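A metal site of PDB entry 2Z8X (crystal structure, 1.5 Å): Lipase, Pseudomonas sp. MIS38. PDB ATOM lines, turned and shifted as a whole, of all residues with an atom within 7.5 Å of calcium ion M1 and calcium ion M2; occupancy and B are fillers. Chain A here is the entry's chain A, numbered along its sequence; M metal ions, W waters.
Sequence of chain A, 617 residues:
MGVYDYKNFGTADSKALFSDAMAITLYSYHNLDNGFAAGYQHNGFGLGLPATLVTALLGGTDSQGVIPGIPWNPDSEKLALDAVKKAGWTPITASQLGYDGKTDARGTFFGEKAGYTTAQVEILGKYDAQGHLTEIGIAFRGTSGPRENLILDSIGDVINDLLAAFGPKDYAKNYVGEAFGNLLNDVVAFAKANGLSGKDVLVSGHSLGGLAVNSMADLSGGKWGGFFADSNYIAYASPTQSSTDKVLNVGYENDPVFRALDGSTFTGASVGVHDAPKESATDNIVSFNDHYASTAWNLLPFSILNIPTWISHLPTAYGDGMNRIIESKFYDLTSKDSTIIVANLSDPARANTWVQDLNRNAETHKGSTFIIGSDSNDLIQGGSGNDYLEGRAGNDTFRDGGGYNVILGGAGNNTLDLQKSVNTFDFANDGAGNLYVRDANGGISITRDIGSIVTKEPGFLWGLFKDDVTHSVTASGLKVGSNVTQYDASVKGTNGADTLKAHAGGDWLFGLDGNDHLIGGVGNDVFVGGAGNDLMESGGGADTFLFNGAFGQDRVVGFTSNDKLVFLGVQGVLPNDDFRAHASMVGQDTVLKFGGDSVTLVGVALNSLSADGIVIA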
ATOM      1  N   ASN A 249     -22.444 -12.090   4.177  1.00  0.00           N
ATOM      2  CA  ASN A 249     -21.841 -12.850   3.077  1.00  0.00           C
ATOM      3  C   ASN A 249     -22.554 -12.516   1.764  1.00  0.00           C
ATOM      4  O   ASN A 249     -23.672 -12.981   1.521  1.00  0.00           O
ATOM      5  CB  ASN A 249     -21.875 -14.360   3.361  1.00  0.00           C
ATOM      6  CG  ASN A 249     -20.725 -14.825   4.242  1.00  0.00           C
ATOM      7  OD1 ASN A 249     -20.930 -15.352   5.356  1.00  0.00           O
ATOM      8  ND2 ASN A 249     -19.506 -14.610   3.780  1.00  0.00           N
ATOM      9  N   GLU A 253     -25.383 -15.439  -7.077  1.00  0.00           N
ATOM     10  CA  GLU A 253     -25.968 -16.768  -7.021  1.00  0.00           C
ATOM     11  C   GLU A 253     -25.267 -17.742  -7.955  1.00  0.00           C
ATOM     12  O   GLU A 253     -25.095 -18.917  -7.628  1.00  0.00           O
ATOM     13  CB  GLU A 253     -27.445 -16.613  -7.400  1.00  0.00           C
ATOM     14  CG  GLU A 253     -28.239 -17.857  -7.549  1.00  0.00           C
ATOM     15  CD  GLU A 253     -29.671 -17.538  -7.907  1.00  0.00           C
ATOM     16  OE1 GLU A 253     -29.952 -17.289  -9.090  1.00  0.00           O
ATOM     17  OE2 GLU A 253     -30.518 -17.539  -6.996  1.00  0.00           O
ATOM     18  N   ASN A 254     -24.873 -17.229  -9.132  1.00  0.00           N
ATOM     19  CA  ASN A 254     -24.226 -18.049 -10.145  1.00  0.00           C
ATOM     20  C   ASN A 254     -22.704 -18.074 -10.053  1.00  0.00           C
ATOM     21  O   ASN A 254     -22.029 -18.622 -10.932  1.00  0.00           O
ATOM     22  CB  ASN A 254     -24.732 -17.699 -11.562  1.00  0.00           C
ATOM     23  CG  ASN A 254     -24.645 -16.223 -11.881  1.00  0.00           C
ATOM     24  OD1 ASN A 254     -24.886 -15.361 -11.035  1.00  0.00           O
ATOM     25  ND2 ASN A 254     -24.325 -15.915 -13.140  1.00  0.00           N
ATOM     26  N   ARG A 259     -20.662 -19.728  -1.372  1.00  0.00           N
ATOM     27  CA  ARG A 259     -21.462 -20.711  -0.613  1.00  0.00           C
ATOM     28  C   ARG A 259     -21.198 -22.164  -1.030  1.00  0.00           C
ATOM     29  O   ARG A 259     -22.061 -23.036  -0.812  1.00  0.00           O
ATOM     30  CB  ARG A 259     -22.958 -20.418  -0.733  1.00  0.00           C
ATOM     31  CG  ARG A 259     -23.396 -18.979  -0.435  1.00  0.00           C
ATOM     32  CD  ARG A 259     -24.835 -18.772  -0.885  1.00  0.00           C
ATOM     33  NE  ARG A 259     -24.952 -19.007  -2.331  1.00  0.00           N
ATOM     34  CZ  ARG A 259     -26.106 -19.172  -2.983  1.00  0.00           C
ATOM     35  NH1 ARG A 259     -27.268 -19.111  -2.347  1.00  0.00           N
ATOM     36  NH2 ARG A 259     -26.067 -19.418  -4.293  1.00  0.00           N
ATOM     37  N   HIS A 274     -25.238 -25.136  -5.480  1.00  0.00           N
ATOM     38  CA  HIS A 274     -25.325 -25.068  -4.013  1.00  0.00           C
ATOM     39  C   HIS A 274     -26.020 -23.781  -3.596  1.00  0.00           C
ATOM     40  O   HIS A 274     -25.415 -22.875  -3.004  1.00  0.00           O
ATOM     41  CB  HIS A 274     -23.937 -25.207  -3.359  1.00  0.00           C
ATOM     42  CG  HIS A 274     -22.853 -24.501  -4.106  1.00  0.00           C
ATOM     43  ND1 HIS A 274     -22.691 -23.134  -4.067  1.00  0.00           N
ATOM     44  CD2 HIS A 274     -21.873 -24.969  -4.921  1.00  0.00           C
ATOM     45  CE1 HIS A 274     -21.651 -22.793  -4.812  1.00  0.00           C
ATOM     46  NE2 HIS A 274     -21.137 -23.888  -5.344  1.00  0.00           N
ATOM     47  N   ASP A 275     -27.321 -23.739  -3.878  1.00  0.00           N
ATOM     48  CA  ASP A 275     -28.107 -22.524  -3.759  1.00  0.00           C
ATOM     49  C   ASP A 275     -29.148 -22.601  -2.634  1.00  0.00           C
ATOM     50  O   ASP A 275     -30.155 -21.886  -2.678  1.00  0.00           O
ATOM     51  CB  ASP A 275     -28.789 -22.230  -5.103  1.00  0.00           C
ATOM     52  CG  ASP A 275     -29.451 -20.863  -5.131  1.00  0.00           C
ATOM     53  OD1 ASP A 275     -28.888 -19.881  -4.591  1.00  0.00           O
ATOM     54  OD2 ASP A 275     -30.555 -20.771  -5.702  1.00  0.00           O
ATOM     55  N   ALA A 276     -28.919 -23.449  -1.638  1.00  0.00           N
ATOM     56  CA  ALA A 276     -29.823 -23.499  -0.505  1.00  0.00           C
ATOM     57  C   ALA A 276     -29.709 -22.187   0.287  1.00  0.00           C
ATOM     58  O   ALA A 276     -28.621 -21.654   0.444  1.00  0.00           O
ATOM     59  CB  ALA A 276     -29.482 -24.690   0.387  1.00  0.00           C
ATOM     60  N   PRO A 277     -30.853 -21.674   0.781  1.00  0.00           N
ATOM     61  CA  PRO A 277     -30.785 -20.432   1.552  1.00  0.00           C
ATOM     62  C   PRO A 277     -29.824 -20.512   2.751  1.00  0.00           C
ATOM     63  O   PRO A 277     -29.735 -21.554   3.424  1.00  0.00           O
ATOM     64  CB  PRO A 277     -32.225 -20.238   2.028  1.00  0.00           C
ATOM     65  CG  PRO A 277     -33.035 -20.918   0.972  1.00  0.00           C
ATOM     66  CD  PRO A 277     -32.241 -22.139   0.636  1.00  0.00           C
ATOM     67  N   LYS A 278     -29.115 -19.423   2.995  1.00  0.00           N
ATOM     68  CA  LYS A 278     -28.216 -19.310   4.141  1.00  0.00           C
ATOM     69  C   LYS A 278     -28.456 -17.993   4.856  1.00  0.00           C
ATOM     70  O   LYS A 278     -28.541 -16.934   4.216  1.00  0.00           O
ATOM     71  CB  LYS A 278     -26.758 -19.431   3.681  1.00  0.00           C
ATOM     72  CG  LYS A 278     -26.394 -20.863   3.275  1.00  0.00           C
ATOM     73  CD  LYS A 278     -24.975 -20.991   2.708  1.00  0.00           C
ATOM     74  CE  LYS A 278     -24.526 -22.460   2.668  1.00  0.00           C
ATOM     75  NZ  LYS A 278     -25.462 -23.290   1.861  1.00  0.00           N
ATOM     76  N   GLU A 279     -28.565 -18.055   6.179  1.00  0.00           N
ATOM     77  CA  GLU A 279     -28.940 -16.901   6.976  1.00  0.00           C
ATOM     78  C   GLU A 279     -27.989 -15.706   6.779  1.00  0.00           C
ATOM     79  O   GLU A 279     -28.411 -14.560   6.713  1.00  0.00           O
ATOM     80  CB  GLU A 279     -29.044 -17.293   8.448  1.00  0.00           C
ATOM     81  CG  GLU A 279     -29.580 -16.209   9.360  1.00  0.00           C
ATOM     82  CD  GLU A 279     -28.506 -15.261   9.876  1.00  0.00           C
ATOM     83  OE1 GLU A 279     -27.314 -15.645   9.881  1.00  0.00           O
ATOM     84  OE2 GLU A 279     -28.866 -14.125  10.290  1.00  0.00           O
ATOM     85  N   SER A 280     -26.689 -15.986   6.704  1.00  0.00           N
ATOM     86  CA  SER A 280     -25.725 -14.886   6.597  1.00  0.00           C
ATOM     87  C   SER A 280     -25.602 -14.321   5.177  1.00  0.00           C
ATOM     88  O   SER A 280     -24.990 -13.268   4.997  1.00  0.00           O
ATOM     89  CB  SER A 280     -24.338 -15.341   7.066  1.00  0.00           C
ATOM     90  OG  SER A 280     -23.764 -16.247   6.142  1.00  0.00           O
ATOM     91  N   ALA A 281     -26.181 -15.011   4.203  1.00  0.00           N
ATOM     92  CA  ALA A 281     -25.862 -14.743   2.799  1.00  0.00           C
ATOM     93  C   ALA A 281     -27.003 -14.110   1.991  1.00  0.00           C
ATOM     94  O   ALA A 281     -28.183 -14.396   2.233  1.00  0.00           O
ATOM     95  CB  ALA A 281     -25.430 -16.025   2.113  1.00  0.00           C
ATOM     96  N   THR A 282     -26.620 -13.287   1.021  1.00  0.00           N
ATOM     97  CA  THR A 282     -27.548 -12.808  -0.013  1.00  0.00           C
ATOM     98  C   THR A 282     -27.694 -13.926  -1.030  1.00  0.00           C
ATOM     99  O   THR A 282     -26.751 -14.229  -1.762  1.00  0.00           O
ATOM    100  CB  THR A 282     -26.979 -11.564  -0.734  1.00  0.00           C
ATOM    101  OG1 THR A 282     -25.668 -11.854  -1.252  1.00  0.00           O
ATOM    102  CG2 THR A 282     -26.894 -10.368   0.219  1.00  0.00           C
ATOM    103  N   ASP A 283     -28.863 -14.544  -1.092  1.00  0.00           N
ATOM    104  CA  ASP A 283     -28.994 -15.794  -1.842  1.00  0.00           C
ATOM    105  C   ASP A 283     -29.475 -15.718  -3.281  1.00  0.00           C
ATOM    106  O   ASP A 283     -29.442 -16.733  -3.993  1.00  0.00           O
ATOM    107  CB  ASP A 283     -29.823 -16.797  -1.047  1.00  0.00           C
ATOM    108  CG  ASP A 283     -29.088 -17.296   0.182  1.00  0.00           C
ATOM    109  OD1 ASP A 283     -27.933 -17.773   0.064  1.00  0.00           O
ATOM    110  OD2 ASP A 283     -29.674 -17.236   1.281  1.00  0.00           O
ATOM    111  N   ASN A 284     -29.898 -14.552  -3.747  1.00  0.00           N
ATOM    112  CA  ASN A 284     -30.601 -14.468  -5.025  1.00  0.00           C
ATOM    113  C   ASN A 284     -30.208 -13.281  -5.921  1.00  0.00           C
ATOM    114  O   ASN A 284     -31.044 -12.710  -6.610  1.00  0.00           O
ATOM    115  CB  ASN A 284     -32.114 -14.474  -4.808  1.00  0.00           C
ATOM    116  CG  ASN A 284     -32.562 -15.679  -3.982  1.00  0.00           C
ATOM    117  OD1 ASN A 284     -32.399 -16.793  -4.403  1.00  0.00           O
ATOM    118  ND2 ASN A 284     -33.129 -15.424  -2.822  1.00  0.00           N
ATOM    119  N   ILE A 285     -28.935 -12.915  -5.867  1.00  0.00           N
ATOM    120  CA  ILE A 285     -28.406 -11.874  -6.746  1.00  0.00           C
ATOM    121  C   ILE A 285     -27.730 -12.538  -7.936  1.00  0.00           C
ATOM    122  O   ILE A 285     -26.719 -13.228  -7.772  1.00  0.00           O
ATOM    123  CB  ILE A 285     -27.393 -10.929  -6.034  1.00  0.00           C
ATOM    124  CG1 ILE A 285     -27.968 -10.376  -4.729  1.00  0.00           C
ATOM    125  CG2 ILE A 285     -26.998  -9.790  -6.962  1.00  0.00           C
ATOM    126  CD1 ILE A 285     -26.971  -9.550  -3.905  1.00  0.00           C
ATOM    127  N   VAL A 286     -28.295 -12.350  -9.128  1.00  0.00           N
ATOM    128  CA  VAL A 286     -27.786 -13.001 -10.347  1.00  0.00           C
ATOM    129  C   VAL A 286     -26.884 -12.067 -11.137  1.00  0.00           C
ATOM    130  O   VAL A 286     -27.230 -10.906 -11.386  1.00  0.00           O
ATOM    131  CB  VAL A 286     -28.968 -13.443 -11.257  1.00  0.00           C
ATOM    132  CG1 VAL A 286     -28.486 -13.994 -12.605  1.00  0.00           C
ATOM    133  CG2 VAL A 286     -29.828 -14.458 -10.537  1.00  0.00           C
ATOM    134  N   LYS A 336     -32.345  -8.786   2.069  1.00  0.00           N
ATOM    135  CA  LYS A 336     -31.158  -9.643   1.923  1.00  0.00           C
ATOM    136  C   LYS A 336     -31.319 -10.710   0.849  1.00  0.00           C
ATOM    137  O   LYS A 336     -30.380 -10.969   0.077  1.00  0.00           O
ATOM    138  CB  LYS A 336     -30.838 -10.294   3.277  1.00  0.00           C
ATOM    139  CG  LYS A 336     -29.474 -10.913   3.384  1.00  0.00           C
ATOM    140  CD  LYS A 336     -29.149 -11.056   4.858  1.00  0.00           C
ATOM    141  CE  LYS A 336     -27.838 -11.749   5.076  1.00  0.00           C
ATOM    142  NZ  LYS A 336     -27.406 -11.507   6.487  1.00  0.00           N
ATOM    143  N   ASP A 337     -32.506 -11.308   0.773  1.00  0.00           N
ATOM    144  CA  ASP A 337     -32.748 -12.401  -0.176  1.00  0.00           C
ATOM    145  C   ASP A 337     -33.675 -12.023  -1.349  1.00  0.00           C
ATOM    146  O   ASP A 337     -34.230 -12.897  -2.007  1.00  0.00           O
ATOM    147  CB  ASP A 337     -33.219 -13.666   0.549  1.00  0.00           C
ATOM    148  CG  ASP A 337     -32.117 -14.289   1.386  1.00  0.00           C
ATOM    149  OD1 ASP A 337     -30.944 -14.273   0.932  1.00  0.00           O
ATOM    150  OD2 ASP A 337     -32.393 -14.784   2.511  1.00  0.00           O
ATOM    151  N   THR A 339     -34.680 -11.156  -5.069  1.00  0.00           N
ATOM    152  CA  THR A 339     -34.177 -11.586  -6.361  1.00  0.00           C
ATOM    153  C   THR A 339     -33.749 -10.347  -7.139  1.00  0.00           C
ATOM    154  O   THR A 339     -34.587  -9.510  -7.485  1.00  0.00           O
ATOM    155  CB  THR A 339     -35.276 -12.282  -7.164  1.00  0.00           C
ATOM    156  OG1 THR A 339     -35.848 -13.337  -6.377  1.00  0.00           O
ATOM    157  CG2 THR A 339     -34.713 -12.837  -8.485  1.00  0.00           C
ATOM    158  N   ASN A 359     -33.637 -17.952 -14.057  1.00  0.00           N
ATOM    159  CA  ASN A 359     -33.671 -18.872 -12.910  1.00  0.00           C
ATOM    160  C   ASN A 359     -32.801 -20.112 -13.149  1.00  0.00           C
ATOM    161  O   ASN A 359     -33.080 -21.181 -12.614  1.00  0.00           O
ATOM    162  CB  ASN A 359     -35.110 -19.290 -12.560  1.00  0.00           C
ATOM    163  CG  ASN A 359     -35.332 -19.442 -11.042  1.00  0.00           C
ATOM    164  OD1 ASN A 359     -36.304 -18.920 -10.503  1.00  0.00           O
ATOM    165  ND2 ASN A 359     -34.426 -20.147 -10.364  1.00  0.00           N
ATOM    166  N   ASN A 361     -29.762 -22.678 -12.817  1.00  0.00           N
ATOM    167  CA  ASN A 361     -28.827 -23.169 -11.786  1.00  0.00           C
ATOM    168  C   ASN A 361     -29.076 -22.548 -10.418  1.00  0.00           C
ATOM    169  O   ASN A 361     -28.168 -22.060  -9.736  1.00  0.00           O
ATOM    170  CB  ASN A 361     -27.383 -22.905 -12.232  1.00  0.00           C
ATOM    171  CG  ASN A 361     -27.007 -23.685 -13.450  1.00  0.00           C
ATOM    172  OD1 ASN A 361     -27.389 -24.848 -13.576  1.00  0.00           O
ATOM    173  ND2 ASN A 361     -26.269 -23.064 -14.356  1.00  0.00           N
ATOM    174  N   ALA A 362     -30.341 -22.575 -10.019  1.00  0.00           N
ATOM    175  CA  ALA A 362     -30.773 -21.932  -8.794  1.00  0.00           C
ATOM    176  C   ALA A 362     -32.115 -22.488  -8.361  1.00  0.00           C
ATOM    177  O   ALA A 362     -32.909 -22.938  -9.195  1.00  0.00           O
ATOM    178  CB  ALA A 362     -30.874 -20.422  -9.003  1.00  0.00           C
ATOM    179  N   GLU A 363     -32.374 -22.416  -7.069  1.00  0.00           N
ATOM    180  CA  GLU A 363     -33.687 -22.749  -6.535  1.00  0.00           C
ATOM    181  C   GLU A 363     -34.707 -21.736  -7.081  1.00  0.00           C
ATOM    182  O   GLU A 363     -34.333 -20.628  -7.478  1.00  0.00           O
ATOM    183  CB  GLU A 363     -33.638 -22.807  -5.005  1.00  0.00           C
ATOM    184  CG  GLU A 363     -32.551 -23.818  -4.559  1.00  0.00           C
ATOM    185  CD  GLU A 363     -32.630 -24.299  -3.107  1.00  0.00           C
ATOM    186  OE1 GLU A 363     -33.480 -23.812  -2.328  1.00  0.00           O
ATOM    187  OE2 GLU A 363     -31.805 -25.173  -2.747  1.00  0.00           O
ATOM    188  N   THR A 364     -35.982 -22.122  -7.131  1.00  0.00           N
ATOM    189  CA  THR A 364     -37.004 -21.245  -7.683  1.00  0.00           C
ATOM    190  C   THR A 364     -37.051 -19.915  -6.949  1.00  0.00           C
ATOM    191  O   THR A 364     -37.132 -19.885  -5.707  1.00  0.00           O
ATOM    192  CB  THR A 364     -38.386 -21.934  -7.666  1.00  0.00           C
ATOM    193  OG1 THR A 364     -38.291 -23.173  -8.384  1.00  0.00           O
ATOM    194  CG2 THR A 364     -39.449 -21.050  -8.314  1.00  0.00           C
ATOM    195  N   HIS A 365     -36.971 -18.827  -7.702  1.00  0.00           N
ATOM    196  CA  HIS A 365     -37.015 -17.486  -7.109  1.00  0.00           C
ATOM    197  C   HIS A 365     -38.408 -17.166  -6.596  1.00  0.00           C
ATOM    198  O   HIS A 365     -39.415 -17.555  -7.205  1.00  0.00           O
ATOM    199  CB  HIS A 365     -36.544 -16.429  -8.096  1.00  0.00           C
ATOM    200  CG  HIS A 365     -35.087 -16.520  -8.409  1.00  0.00           C
ATOM    201  ND1 HIS A 365     -34.570 -16.243  -9.660  1.00  0.00           N
ATOM    202  CD2 HIS A 365     -34.023 -16.842  -7.631  1.00  0.00           C
ATOM    203  CE1 HIS A 365     -33.257 -16.411  -9.633  1.00  0.00           C
ATOM    204  NE2 HIS A 365     -32.905 -16.774  -8.413  1.00  0.00           N
HETATM  205 CA    CA M   1     -30.861 -18.444  -4.961  1.00  0.00          CA
HETATM  206 CA    CA M   2     -30.109 -15.616   2.902  1.00  0.00          CA
HETATM  207  O   HOH W   1     -30.394 -14.213   4.799  1.00  0.00           O
HETATM  208  O   HOH W   2     -31.565 -17.257   3.986  1.00  0.00           O
HETATM  209  O   HOH W   3     -33.022 -19.081  -5.625  1.00  0.00           O
HETATM  210  O   HOH W   4     -31.307 -19.430  -2.777  1.00  0.00           O
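Calcium ion M2 is bound by the side-chain carboxylate (OD2) of Asp 283 (2.3 Å), the backbone carbonyl oxygen (O) of Ala 281 (2.4 Å), water W1 (2.4 Å), the backbone carbonyl oxygen (O) of Lys 278 (2.4 Å), water W2 (2.4 Å), the side-chain carboxylate (OD2) of Asp 337 (2.5 Å) and the side-chain carboxylate (OD1) of Asp 337 (2.5 Å). Calcium ion M2 has seven donor atoms within binding distance.
The side-chain carboxylate (OE1) of Glu 253 lies within hydrogen-bond range of a ring nitrogen (NE2) of His 365, at 3.1 Å. The backbone carbonyl oxygen (O) of Ile 285 is in hydrogen-bond range of the backbone NH (N) of Glu 253, 2.7 Å away. The backbone carbonyl oxygen (O) of Asp 337 is in hydrogen-bond range of the side-chain amide nitrogen (ND2) of Asn 284 (2.9 Å). NH1 of Arg 259 is in salt-bridge range of OD1 of Asp 283, at 2.8 Å. NH1 of Arg 259 sits close to OD1 of Asp 275 (2.9 Å). The backbone NH (N) of Glu 363 lies close to the side-chain carboxylate (OD2) of Asp 275 (2.8 Å).
Calcium ion M1 is bound by the side-chain carboxylate (OE2) of Glu 253 (2.3 Å), the side-chain amide oxygen (OD1) of Asn 284 (2.3 Å), water W3 (2.3 Å), the backbone carbonyl oxygen (O) of Asp 283 (2.4 Å), water W4 (2.4 Å), the side-chain carboxylate (OD2) of Asp 275 (2.5 Å) and the side-chain carboxylate (OD1) of Asp 275 (2.5 Å). Calcium ion M1 has seven donor atoms within binding distance.
Within 4 Å of calcium ion M2: Lys 278, Ala 281, Asp 283 and Asp 337.
Four residues have an atom within 4 Å of calcium ion M1: Glu 253, Asp 275, Asp 283 and Asn 284. Along chain A the residues within 4 Å of calcium ion M1 span positions 253 to 284. The nearest printed residue that does not touch calcium ion M1 is His 365 (4.3 Å).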
